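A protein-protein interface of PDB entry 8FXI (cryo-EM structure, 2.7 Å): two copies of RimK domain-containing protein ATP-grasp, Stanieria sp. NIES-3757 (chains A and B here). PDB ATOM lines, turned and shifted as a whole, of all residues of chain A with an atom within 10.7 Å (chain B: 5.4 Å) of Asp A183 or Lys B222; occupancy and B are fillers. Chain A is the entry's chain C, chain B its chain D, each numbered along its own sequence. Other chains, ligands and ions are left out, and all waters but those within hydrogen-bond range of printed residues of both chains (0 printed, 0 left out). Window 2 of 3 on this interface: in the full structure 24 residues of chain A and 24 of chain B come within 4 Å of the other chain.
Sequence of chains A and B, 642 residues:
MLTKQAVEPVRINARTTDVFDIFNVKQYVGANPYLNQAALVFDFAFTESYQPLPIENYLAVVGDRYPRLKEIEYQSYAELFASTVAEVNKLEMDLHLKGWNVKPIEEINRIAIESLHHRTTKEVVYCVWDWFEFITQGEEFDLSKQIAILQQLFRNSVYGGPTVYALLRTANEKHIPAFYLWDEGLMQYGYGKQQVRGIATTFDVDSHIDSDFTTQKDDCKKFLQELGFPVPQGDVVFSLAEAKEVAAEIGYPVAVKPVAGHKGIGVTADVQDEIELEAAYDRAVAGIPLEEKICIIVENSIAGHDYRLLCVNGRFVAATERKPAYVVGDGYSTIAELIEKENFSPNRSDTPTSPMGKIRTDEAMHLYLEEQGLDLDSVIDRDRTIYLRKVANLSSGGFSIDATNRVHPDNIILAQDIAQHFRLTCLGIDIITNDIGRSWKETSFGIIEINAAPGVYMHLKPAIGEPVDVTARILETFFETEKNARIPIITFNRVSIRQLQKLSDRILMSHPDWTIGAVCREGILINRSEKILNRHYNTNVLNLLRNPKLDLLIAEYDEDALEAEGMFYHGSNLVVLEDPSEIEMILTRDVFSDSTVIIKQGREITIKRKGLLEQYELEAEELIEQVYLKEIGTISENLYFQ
Of the 19 printed residues of chain A, 4 touch a printed residue of chain B.
Of the 10 printed residues of chain B, 4 touch a printed residue of chain A.
Hydrophobic or aromatic side chains of chain B within 4 Å of the printed part of chain A: Phe B213 and Phe B223.
Among the printed residues, no Asp or Glu carboxylate lies within 4 Å of a Lys or Arg side-chain nitrogen of the other chain.
OD1 of Asn A543 lies close to O of Thr A539, 3.3 Å away.
The backbone NH (N) of Asn A534 is in hydrogen-bond range of the side-chain amide oxygen (OD1) of Asn A540, at 3.2 Å.
The side-chain amide oxygen (OD1) of Asn A534 sits at hydrogen-bond distance from the backbone NH (N) of His A536 (3.4 Å).
The side-chain carboxylate (OE2) of Glu A184 is in salt-bridge range of the guanidinium group (NH2) of Arg A546, at 3.6 Å.
The side-chain amide nitrogen (ND2) of Asn A534 is in hydrogen-bond range of the side-chain hydroxyl (OG1) of Thr A539 (3.2 Å).
The side-chain amino group (NZ) of Lys B222 lies within salt-bridge range of the side-chain carboxylate (OE2) of Glu B226, 3.6 Å away.
Of chain B, only Lys B222 comes within 4 Å of Asp A183.
Lys B222 touches just one residue of chain A: Asp A183 (3.97 Å).
Asp B219 touches none of the printed residues of chain A.
Cys B220 touches none of the printed residues of chain A.
No residue of chain A comes within 4 Å of Gln B225.
Of the printed residues of chain A, Phe B223 touches Glu A184 (3.7 Å).
Of the printed residues of chain B, Asn A543 touches Glu B226.
Printed residues of chain B within 4 Å of Asn A534: Glu B226.
Of the printed residues of chain B, Glu A184 touches Phe B213 and Phe B223.
Of the printed residues of chain A, Phe B213 touches Glu A184.
The nearest residue of chain B that does not touch Asp A183 is Phe B213 (4.2 Å).
The nearest printed residue of chain A that does not touch Phe B223 is Arg A546 (4.3 Å).
No position is printed for both chains.
Of the 5 pairs that touch across the chains among the printed residues, none has its exchanged pair printed and touching as well.
Among the printed residues, merely in contact across the chains: Asp A183 with Lys B222 (3.97 Å), Glu A184 with Phe B213 (3.5 Å), Glu A184 with Phe B223 (3.7 Å) and Asn A534 with Glu B226 (3.7 Å).
The backbone carbonyl oxygen of Glu B226 lies within hydrogen-bond range of the side-chain amide nitrogen of Asn A543 (3.2 Å).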
ATOM      1  N   VAL A 158       7.518 -17.451 -24.283  1.00  0.00           N
ATOM      2  CA  VAL A 158       7.254 -18.860 -24.544  1.00  0.00           C
ATOM      3  C   VAL A 158       8.289 -19.487 -25.459  1.00  0.00           C
ATOM      4  O   VAL A 158       8.205 -20.688 -25.741  1.00  0.00           O
ATOM      5  CB  VAL A 158       5.846 -19.045 -25.138  1.00  0.00           C
ATOM      6  CG1 VAL A 158       4.808 -18.516 -24.181  1.00  0.00           C
ATOM      7  CG2 VAL A 158       5.740 -18.337 -26.460  1.00  0.00           C
ATOM      8  N   PHE A 179       5.815 -25.521 -34.157  1.00  0.00           N
ATOM      9  CA  PHE A 179       5.055 -24.293 -33.949  1.00  0.00           C
ATOM     10  C   PHE A 179       4.263 -24.377 -32.653  1.00  0.00           C
ATOM     11  O   PHE A 179       4.000 -25.459 -32.132  1.00  0.00           O
ATOM     12  CB  PHE A 179       4.132 -23.996 -35.133  1.00  0.00           C
ATOM     13  CG  PHE A 179       3.187 -25.107 -35.465  1.00  0.00           C
ATOM     14  CD1 PHE A 179       3.578 -26.144 -36.286  1.00  0.00           C
ATOM     15  CD2 PHE A 179       1.901 -25.105 -34.970  1.00  0.00           C
ATOM     16  CE1 PHE A 179       2.707 -27.162 -36.591  1.00  0.00           C
ATOM     17  CE2 PHE A 179       1.029 -26.120 -35.273  1.00  0.00           C
ATOM     18  CZ  PHE A 179       1.431 -27.147 -36.085  1.00  0.00           C
ATOM     19  N   TYR A 180       3.870 -23.211 -32.152  1.00  0.00           N
ATOM     20  CA  TYR A 180       3.252 -23.070 -30.840  1.00  0.00           C
ATOM     21  C   TYR A 180       1.733 -23.045 -30.953  1.00  0.00           C
ATOM     22  O   TYR A 180       1.183 -22.467 -31.891  1.00  0.00           O
ATOM     23  CB  TYR A 180       3.746 -21.790 -30.172  1.00  0.00           C
ATOM     24  CG  TYR A 180       3.403 -21.665 -28.713  1.00  0.00           C
ATOM     25  CD1 TYR A 180       4.161 -22.298 -27.749  1.00  0.00           C
ATOM     26  CD2 TYR A 180       2.334 -20.901 -28.299  1.00  0.00           C
ATOM     27  CE1 TYR A 180       3.852 -22.183 -26.418  1.00  0.00           C
ATOM     28  CE2 TYR A 180       2.020 -20.780 -26.971  1.00  0.00           C
ATOM     29  CZ  TYR A 180       2.781 -21.421 -26.036  1.00  0.00           C
ATOM     30  OH  TYR A 180       2.466 -21.298 -24.707  1.00  0.00           O
ATOM     31  N   LEU A 181       1.054 -23.665 -29.986  1.00  0.00           N
ATOM     32  CA  LEU A 181      -0.404 -23.738 -29.966  1.00  0.00           C
ATOM     33  C   LEU A 181      -0.932 -22.789 -28.897  1.00  0.00           C
ATOM     34  O   LEU A 181      -0.817 -23.071 -27.702  1.00  0.00           O
ATOM     35  CB  LEU A 181      -0.868 -25.167 -29.697  1.00  0.00           C
ATOM     36  CG  LEU A 181      -0.424 -26.260 -30.672  1.00  0.00           C
ATOM     37  CD1 LEU A 181      -0.782 -27.622 -30.133  1.00  0.00           C
ATOM     38  CD2 LEU A 181      -1.054 -26.061 -32.026  1.00  0.00           C
ATOM     39  N   TRP A 182      -1.526 -21.673 -29.322  1.00  0.00           N
ATOM     40  CA  TRP A 182      -1.980 -20.657 -28.379  1.00  0.00           C
ATOM     41  C   TRP A 182      -3.354 -20.958 -27.805  1.00  0.00           C
ATOM     42  O   TRP A 182      -4.192 -20.058 -27.704  1.00  0.00           O
ATOM     43  CB  TRP A 182      -2.042 -19.287 -29.057  1.00  0.00           C
ATOM     44  CG  TRP A 182      -0.740 -18.613 -29.255  1.00  0.00           C
ATOM     45  CD1 TRP A 182       0.013 -18.605 -30.386  1.00  0.00           C
ATOM     46  CD2 TRP A 182      -0.040 -17.819 -28.300  1.00  0.00           C
ATOM     47  NE1 TRP A 182       1.149 -17.864 -30.192  1.00  0.00           N
ATOM     48  CE2 TRP A 182       1.139 -17.370 -28.915  1.00  0.00           C
ATOM     49  CE3 TRP A 182      -0.292 -17.450 -26.978  1.00  0.00           C
ATOM     50  CZ2 TRP A 182       2.063 -16.571 -28.257  1.00  0.00           C
ATOM     51  CZ3 TRP A 182       0.623 -16.660 -26.326  1.00  0.00           C
ATOM     52  CH2 TRP A 182       1.786 -16.228 -26.965  1.00  0.00           C
ATOM     53  N   ASP A 183      -3.596 -22.198 -27.399  1.00  0.00           N
ATOM     54  CA  ASP A 183      -4.809 -22.537 -26.662  1.00  0.00           C
ATOM     55  C   ASP A 183      -4.563 -23.477 -25.502  1.00  0.00           C
ATOM     56  O   ASP A 183      -5.389 -23.524 -24.586  1.00  0.00           O
ATOM     57  CB  ASP A 183      -5.857 -23.163 -27.586  1.00  0.00           C
ATOM     58  CG  ASP A 183      -6.610 -22.132 -28.396  1.00  0.00           C
ATOM     59  OD1 ASP A 183      -6.834 -21.016 -27.884  1.00  0.00           O
ATOM     60  OD2 ASP A 183      -6.985 -22.435 -29.544  1.00  0.00           O
ATOM     61  N   GLU A 184      -3.467 -24.227 -25.506  1.00  0.00           N
ATOM     62  CA  GLU A 184      -3.141 -25.149 -24.438  1.00  0.00           C
ATOM     63  C   GLU A 184      -1.699 -25.030 -23.976  1.00  0.00           C
ATOM     64  O   GLU A 184      -1.280 -25.807 -23.114  1.00  0.00           O
ATOM     65  CB  GLU A 184      -3.425 -26.584 -24.882  1.00  0.00           C
ATOM     66  CG  GLU A 184      -3.212 -26.809 -26.359  1.00  0.00           C
ATOM     67  CD  GLU A 184      -4.069 -27.931 -26.894  1.00  0.00           C
ATOM     68  OE1 GLU A 184      -5.244 -28.014 -26.496  1.00  0.00           O
ATOM     69  OE2 GLU A 184      -3.573 -28.733 -27.708  1.00  0.00           O
ATOM     70  N   GLY A 185      -0.939 -24.076 -24.503  1.00  0.00           N
ATOM     71  CA  GLY A 185       0.421 -23.863 -24.062  1.00  0.00           C
ATOM     72  C   GLY A 185       1.368 -24.996 -24.385  1.00  0.00           C
ATOM     73  O   GLY A 185       2.140 -25.424 -23.524  1.00  0.00           O
ATOM     74  N   LEU A 186       1.324 -25.490 -25.617  1.00  0.00           N
ATOM     75  CA  LEU A 186       2.181 -26.582 -26.044  1.00  0.00           C
ATOM     76  C   LEU A 186       2.900 -26.216 -27.331  1.00  0.00           C
ATOM     77  O   LEU A 186       2.565 -25.240 -28.007  1.00  0.00           O
ATOM     78  CB  LEU A 186       1.387 -27.872 -26.260  1.00  0.00           C
ATOM     79  CG  LEU A 186       0.618 -28.473 -25.091  1.00  0.00           C
ATOM     80  CD1 LEU A 186      -0.003 -29.773 -25.524  1.00  0.00           C
ATOM     81  CD2 LEU A 186       1.524 -28.697 -23.911  1.00  0.00           C
ATOM     82  N   MET A 187       3.899 -27.025 -27.659  1.00  0.00           N
ATOM     83  CA  MET A 187       4.664 -26.916 -28.890  1.00  0.00           C
ATOM     84  C   MET A 187       4.489 -28.204 -29.680  1.00  0.00           C
ATOM     85  O   MET A 187       4.484 -29.290 -29.102  1.00  0.00           O
ATOM     86  CB  MET A 187       6.140 -26.675 -28.580  1.00  0.00           C
ATOM     87  CG  MET A 187       7.006 -26.336 -29.769  1.00  0.00           C
ATOM     88  SD  MET A 187       6.949 -24.599 -30.219  1.00  0.00           S
ATOM     89  CE  MET A 187       7.363 -23.826 -28.666  1.00  0.00           C
ATOM     90  N   GLN A 188       4.334 -28.091 -30.997  1.00  0.00           N
ATOM     91  CA  GLN A 188       4.115 -29.252 -31.853  1.00  0.00           C
ATOM     92  C   GLN A 188       5.283 -29.391 -32.818  1.00  0.00           C
ATOM     93  O   GLN A 188       5.815 -28.385 -33.304  1.00  0.00           O
ATOM     94  CB  GLN A 188       2.797 -29.144 -32.606  1.00  0.00           C
ATOM     95  CG  GLN A 188       2.522 -30.364 -33.445  1.00  0.00           C
ATOM     96  CD  GLN A 188       1.148 -30.377 -34.032  1.00  0.00           C
ATOM     97  OE1 GLN A 188       0.215 -29.831 -33.463  1.00  0.00           O
ATOM     98  NE2 GLN A 188       1.012 -31.000 -35.187  1.00  0.00           N
ATOM     99  N   ARG A 197       3.563 -33.678 -29.365  1.00  0.00           N
ATOM    100  CA  ARG A 197       3.291 -32.467 -28.603  1.00  0.00           C
ATOM    101  C   ARG A 197       3.922 -32.555 -27.222  1.00  0.00           C
ATOM    102  O   ARG A 197       3.936 -33.623 -26.609  1.00  0.00           O
ATOM    103  CB  ARG A 197       1.789 -32.239 -28.459  1.00  0.00           C
ATOM    104  CG  ARG A 197       1.069 -32.088 -29.766  1.00  0.00           C
ATOM    105  CD  ARG A 197      -0.419 -31.972 -29.565  1.00  0.00           C
ATOM    106  NE  ARG A 197      -1.018 -33.237 -29.164  1.00  0.00           N
ATOM    107  CZ  ARG A 197      -1.636 -33.444 -28.012  1.00  0.00           C
ATOM    108  NH1 ARG A 197      -1.768 -32.482 -27.117  1.00  0.00           N
ATOM    109  NH2 ARG A 197      -2.143 -34.644 -27.754  1.00  0.00           N
ATOM    110  N   ASN A 534     -14.234 -21.073 -40.378  1.00  0.00           N
ATOM    111  CA  ASN A 534     -13.918 -20.028 -39.417  1.00  0.00           C
ATOM    112  C   ASN A 534     -13.783 -18.673 -40.108  1.00  0.00           C
ATOM    113  O   ASN A 534     -13.542 -18.581 -41.312  1.00  0.00           O
ATOM    114  CB  ASN A 534     -12.628 -20.371 -38.673  1.00  0.00           C
ATOM    115  CG  ASN A 534     -12.494 -19.635 -37.360  1.00  0.00           C
ATOM    116  OD1 ASN A 534     -12.884 -18.477 -37.240  1.00  0.00           O
ATOM    117  ND2 ASN A 534     -11.942 -20.307 -36.363  1.00  0.00           N
ATOM    118  N   HIS A 536     -11.458 -16.242 -39.351  1.00  0.00           N
ATOM    119  CA  HIS A 536     -10.046 -15.982 -39.599  1.00  0.00           C
ATOM    120  C   HIS A 536      -9.490 -17.118 -40.445  1.00  0.00           C
ATOM    121  O   HIS A 536      -9.500 -18.274 -40.016  1.00  0.00           O
ATOM    122  CB  HIS A 536      -9.293 -15.858 -38.278  1.00  0.00           C
ATOM    123  CG  HIS A 536      -7.877 -15.406 -38.426  1.00  0.00           C
ATOM    124  ND1 HIS A 536      -6.803 -16.207 -38.105  1.00  0.00           N
ATOM    125  CD2 HIS A 536      -7.356 -14.233 -38.853  1.00  0.00           C
ATOM    126  CE1 HIS A 536      -5.682 -15.549 -38.334  1.00  0.00           C
ATOM    127  NE2 HIS A 536      -5.989 -14.348 -38.789  1.00  0.00           N
ATOM    128  N   THR A 539      -6.663 -19.989 -39.412  1.00  0.00           N
ATOM    129  CA  THR A 539      -6.850 -20.974 -38.352  1.00  0.00           C
ATOM    130  C   THR A 539      -7.384 -22.298 -38.877  1.00  0.00           C
ATOM    131  O   THR A 539      -7.216 -23.327 -38.218  1.00  0.00           O
ATOM    132  CB  THR A 539      -7.784 -20.438 -37.272  1.00  0.00           C
ATOM    133  OG1 THR A 539      -9.064 -20.163 -37.841  1.00  0.00           O
ATOM    134  CG2 THR A 539      -7.224 -19.174 -36.671  1.00  0.00           C
ATOM    135  N   ASN A 540      -8.029 -22.300 -40.040  1.00  0.00           N
ATOM    136  CA  ASN A 540      -8.511 -23.555 -40.605  1.00  0.00           C
ATOM    137  C   ASN A 540      -7.355 -24.480 -40.960  1.00  0.00           C
ATOM    138  O   ASN A 540      -7.426 -25.694 -40.729  1.00  0.00           O
ATOM    139  CB  ASN A 540      -9.371 -23.275 -41.831  1.00  0.00           C
ATOM    140  CG  ASN A 540     -10.502 -22.323 -41.539  1.00  0.00           C
ATOM    141  OD1 ASN A 540     -11.512 -22.704 -40.960  1.00  0.00           O
ATOM    142  ND2 ASN A 540     -10.342 -21.078 -41.945  1.00  0.00           N
ATOM    143  N   LEU A 542      -4.418 -24.528 -39.526  1.00  0.00           N
ATOM    144  CA  LEU A 542      -3.890 -25.029 -38.263  1.00  0.00           C
ATOM    145  C   LEU A 542      -4.764 -26.142 -37.701  1.00  0.00           C
ATOM    146  O   LEU A 542      -4.254 -27.154 -37.207  1.00  0.00           O
ATOM    147  CB  LEU A 542      -3.769 -23.879 -37.267  1.00  0.00           C
ATOM    148  CG  LEU A 542      -3.245 -24.171 -35.864  1.00  0.00           C
ATOM    149  CD1 LEU A 542      -2.381 -23.031 -35.397  1.00  0.00           C
ATOM    150  CD2 LEU A 542      -4.390 -24.364 -34.902  1.00  0.00           C
ATOM    151  N   ASN A 543      -6.084 -25.972 -37.767  1.00  0.00           N
ATOM    152  CA  ASN A 543      -6.988 -27.018 -37.304  1.00  0.00           C
ATOM    153  C   ASN A 543      -6.789 -28.302 -38.091  1.00  0.00           C
ATOM    154  O   ASN A 543      -6.875 -29.399 -37.532  1.00  0.00           O
ATOM    155  CB  ASN A 543      -8.436 -26.552 -37.414  1.00  0.00           C
ATOM    156  CG  ASN A 543      -8.794 -25.512 -36.384  1.00  0.00           C
ATOM    157  OD1 ASN A 543      -7.974 -25.141 -35.549  1.00  0.00           O
ATOM    158  ND2 ASN A 543     -10.024 -25.027 -36.440  1.00  0.00           N
ATOM    159  N   ARG A 546      -3.459 -29.986 -37.017  1.00  0.00           N
ATOM    160  CA  ARG A 546      -3.508 -30.530 -35.665  1.00  0.00           C
ATOM    161  C   ARG A 546      -4.223 -31.879 -35.584  1.00  0.00           C
ATOM    162  O   ARG A 546      -4.055 -32.594 -34.594  1.00  0.00           O
ATOM    163  CB  ARG A 546      -4.173 -29.499 -34.744  1.00  0.00           C
ATOM    164  CG  ARG A 546      -4.596 -29.961 -33.366  1.00  0.00           C
ATOM    165  CD  ARG A 546      -3.429 -30.245 -32.450  1.00  0.00           C
ATOM    166  NE  ARG A 546      -3.883 -30.451 -31.082  1.00  0.00           N
ATOM    167  CZ  ARG A 546      -4.378 -31.590 -30.621  1.00  0.00           C
ATOM    168  NH1 ARG A 546      -4.476 -32.661 -31.387  1.00  0.00           N
ATOM    169  NH2 ARG A 546      -4.787 -31.655 -29.359  1.00  0.00           N
ATOM    170  N   PHE B 213      -5.495 -31.129 -18.939  1.00  0.00           N
ATOM    171  CA  PHE B 213      -6.230 -30.193 -19.779  1.00  0.00           C
ATOM    172  C   PHE B 213      -7.727 -30.293 -19.536  1.00  0.00           C
ATOM    173  O   PHE B 213      -8.421 -29.274 -19.472  1.00  0.00           O
ATOM    174  CB  PHE B 213      -5.913 -30.430 -21.251  1.00  0.00           C
ATOM    175  CG  PHE B 213      -6.457 -29.369 -22.157  1.00  0.00           C
ATOM    176  CD1 PHE B 213      -6.120 -28.044 -21.969  1.00  0.00           C
ATOM    177  CD2 PHE B 213      -7.298 -29.696 -23.200  1.00  0.00           C
ATOM    178  CE1 PHE B 213      -6.614 -27.070 -22.798  1.00  0.00           C
ATOM    179  CE2 PHE B 213      -7.793 -28.722 -24.029  1.00  0.00           C
ATOM    180  CZ  PHE B 213      -7.448 -27.410 -23.829  1.00  0.00           C
ATOM    181  N   ASP B 218     -13.049 -23.650 -18.808  1.00  0.00           N
ATOM    182  CA  ASP B 218     -12.916 -22.312 -19.384  1.00  0.00           C
ATOM    183  C   ASP B 218     -11.734 -22.234 -20.343  1.00  0.00           C
ATOM    184  O   ASP B 218     -11.625 -21.253 -21.082  1.00  0.00           O
ATOM    185  CB  ASP B 218     -12.785 -21.207 -18.321  1.00  0.00           C
ATOM    186  CG  ASP B 218     -11.408 -20.574 -18.293  1.00  0.00           C
ATOM    187  OD1 ASP B 218     -10.507 -21.112 -17.619  1.00  0.00           O
ATOM    188  OD2 ASP B 218     -11.222 -19.529 -18.952  1.00  0.00           O
ATOM    189  N   ASP B 219     -10.877 -23.253 -20.400  1.00  0.00           N
ATOM    190  CA  ASP B 219      -9.829 -23.323 -21.403  1.00  0.00           C
ATOM    191  C   ASP B 219     -10.091 -24.371 -22.467  1.00  0.00           C
ATOM    192  O   ASP B 219      -9.686 -24.172 -23.613  1.00  0.00           O
ATOM    193  CB  ASP B 219      -8.472 -23.612 -20.752  1.00  0.00           C
ATOM    194  CG  ASP B 219      -7.935 -22.428 -19.989  1.00  0.00           C
ATOM    195  OD1 ASP B 219      -8.620 -21.385 -19.962  1.00  0.00           O
ATOM    196  OD2 ASP B 219      -6.831 -22.536 -19.418  1.00  0.00           O
ATOM    197  N   CYS B 220     -10.742 -25.480 -22.118  1.00  0.00           N
ATOM    198  CA  CYS B 220     -11.223 -26.390 -23.147  1.00  0.00           C
ATOM    199  C   CYS B 220     -12.491 -25.857 -23.795  1.00  0.00           C
ATOM    200  O   CYS B 220     -12.851 -26.281 -24.896  1.00  0.00           O
ATOM    201  CB  CYS B 220     -11.455 -27.783 -22.564  1.00  0.00           C
ATOM    202  SG  CYS B 220     -12.438 -27.819 -21.066  1.00  0.00           S
ATOM    203  N   LYS B 221     -13.165 -24.921 -23.131  1.00  0.00           N
ATOM    204  CA  LYS B 221     -14.323 -24.266 -23.725  1.00  0.00           C
ATOM    205  C   LYS B 221     -13.929 -23.490 -24.975  1.00  0.00           C
ATOM    206  O   LYS B 221     -14.560 -23.619 -26.028  1.00  0.00           O
ATOM    207  CB  LYS B 221     -14.960 -23.346 -22.688  1.00  0.00           C
ATOM    208  CG  LYS B 221     -16.290 -22.754 -23.063  1.00  0.00           C
ATOM    209  CD  LYS B 221     -16.845 -21.991 -21.877  1.00  0.00           C
ATOM    210  CE  LYS B 221     -18.159 -21.326 -22.200  1.00  0.00           C
ATOM    211  NZ  LYS B 221     -18.010 -20.347 -23.306  1.00  0.00           N
ATOM    212  N   LYS B 222     -12.861 -22.699 -24.881  1.00  0.00           N
ATOM    213  CA  LYS B 222     -12.384 -21.956 -26.042  1.00  0.00           C
ATOM    214  C   LYS B 222     -11.827 -22.890 -27.109  1.00  0.00           C
ATOM    215  O   LYS B 222     -12.007 -22.658 -28.312  1.00  0.00           O
ATOM    216  CB  LYS B 222     -11.327 -20.946 -25.600  1.00  0.00           C
ATOM    217  CG  LYS B 222     -10.845 -20.038 -26.701  1.00  0.00           C
ATOM    218  CD  LYS B 222      -9.899 -18.982 -26.164  1.00  0.00           C
ATOM    219  CE  LYS B 222      -9.419 -18.068 -27.275  1.00  0.00           C
ATOM    220  NZ  LYS B 222     -10.563 -17.452 -27.997  1.00  0.00           N
ATOM    221  N   PHE B 223     -11.149 -23.957 -26.683  1.00  0.00           N
ATOM    222  CA  PHE B 223     -10.627 -24.935 -27.627  1.00  0.00           C
ATOM    223  C   PHE B 223     -11.749 -25.566 -28.438  1.00  0.00           C
ATOM    224  O   PHE B 223     -11.629 -25.732 -29.654  1.00  0.00           O
ATOM    225  CB  PHE B 223      -9.830 -26.002 -26.878  1.00  0.00           C
ATOM    226  CG  PHE B 223      -9.267 -27.078 -27.758  1.00  0.00           C
ATOM    227  CD1 PHE B 223      -8.129 -26.854 -28.505  1.00  0.00           C
ATOM    228  CD2 PHE B 223      -9.863 -28.321 -27.820  1.00  0.00           C
ATOM    229  CE1 PHE B 223      -7.609 -27.843 -29.309  1.00  0.00           C
ATOM    230  CE2 PHE B 223      -9.346 -29.309 -28.624  1.00  0.00           C
ATOM    231  CZ  PHE B 223      -8.219 -29.070 -29.368  1.00  0.00           C
ATOM    232  N   LEU B 224     -12.855 -25.919 -27.783  1.00  0.00           N
ATOM    233  CA  LEU B 224     -13.991 -26.464 -28.515  1.00  0.00           C
ATOM    234  C   LEU B 224     -14.670 -25.405 -29.369  1.00  0.00           C
ATOM    235  O   LEU B 224     -15.157 -25.712 -30.460  1.00  0.00           O
ATOM    236  CB  LEU B 224     -14.997 -27.083 -27.550  1.00  0.00           C
ATOM    237  CG  LEU B 224     -14.577 -28.346 -26.805  1.00  0.00           C
ATOM    238  CD1 LEU B 224     -15.690 -28.799 -25.892  1.00  0.00           C
ATOM    239  CD2 LEU B 224     -14.218 -29.444 -27.775  1.00  0.00           C
ATOM    240  N   GLN B 225     -14.722 -24.162 -28.893  1.00  0.00           N
ATOM    241  CA  GLN B 225     -15.394 -23.109 -29.645  1.00  0.00           C
ATOM    242  C   GLN B 225     -14.680 -22.796 -30.951  1.00  0.00           C
ATOM    243  O   GLN B 225     -15.330 -22.470 -31.948  1.00  0.00           O
ATOM    244  CB  GLN B 225     -15.504 -21.852 -28.791  1.00  0.00           C
ATOM    245  CG  GLN B 225     -16.039 -20.652 -29.528  1.00  0.00           C
ATOM    246  CD  GLN B 225     -16.053 -19.412 -28.672  1.00  0.00           C
ATOM    247  OE1 GLN B 225     -15.878 -19.482 -27.458  1.00  0.00           O
ATOM    248  NE2 GLN B 225     -16.260 -18.264 -29.302  1.00  0.00           N
ATOM    249  N   GLU B 226     -13.356 -22.896 -30.974  1.00  0.00           N
ATOM    250  CA  GLU B 226     -12.603 -22.585 -32.185  1.00  0.00           C
ATOM    251  C   GLU B 226     -12.699 -23.668 -33.258  1.00  0.00           C
ATOM    252  O   GLU B 226     -11.888 -23.658 -34.186  1.00  0.00           O
ATOM    253  CB  GLU B 226     -11.135 -22.335 -31.845  1.00  0.00           C
ATOM    254  CG  GLU B 226     -10.907 -21.120 -30.977  1.00  0.00           C
ATOM    255  CD  GLU B 226     -11.187 -19.824 -31.704  1.00  0.00           C
ATOM    256  OE1 GLU B 226     -10.816 -19.717 -32.890  1.00  0.00           O
ATOM    257  OE2 GLU B 226     -11.779 -18.912 -31.092  1.00  0.00           O
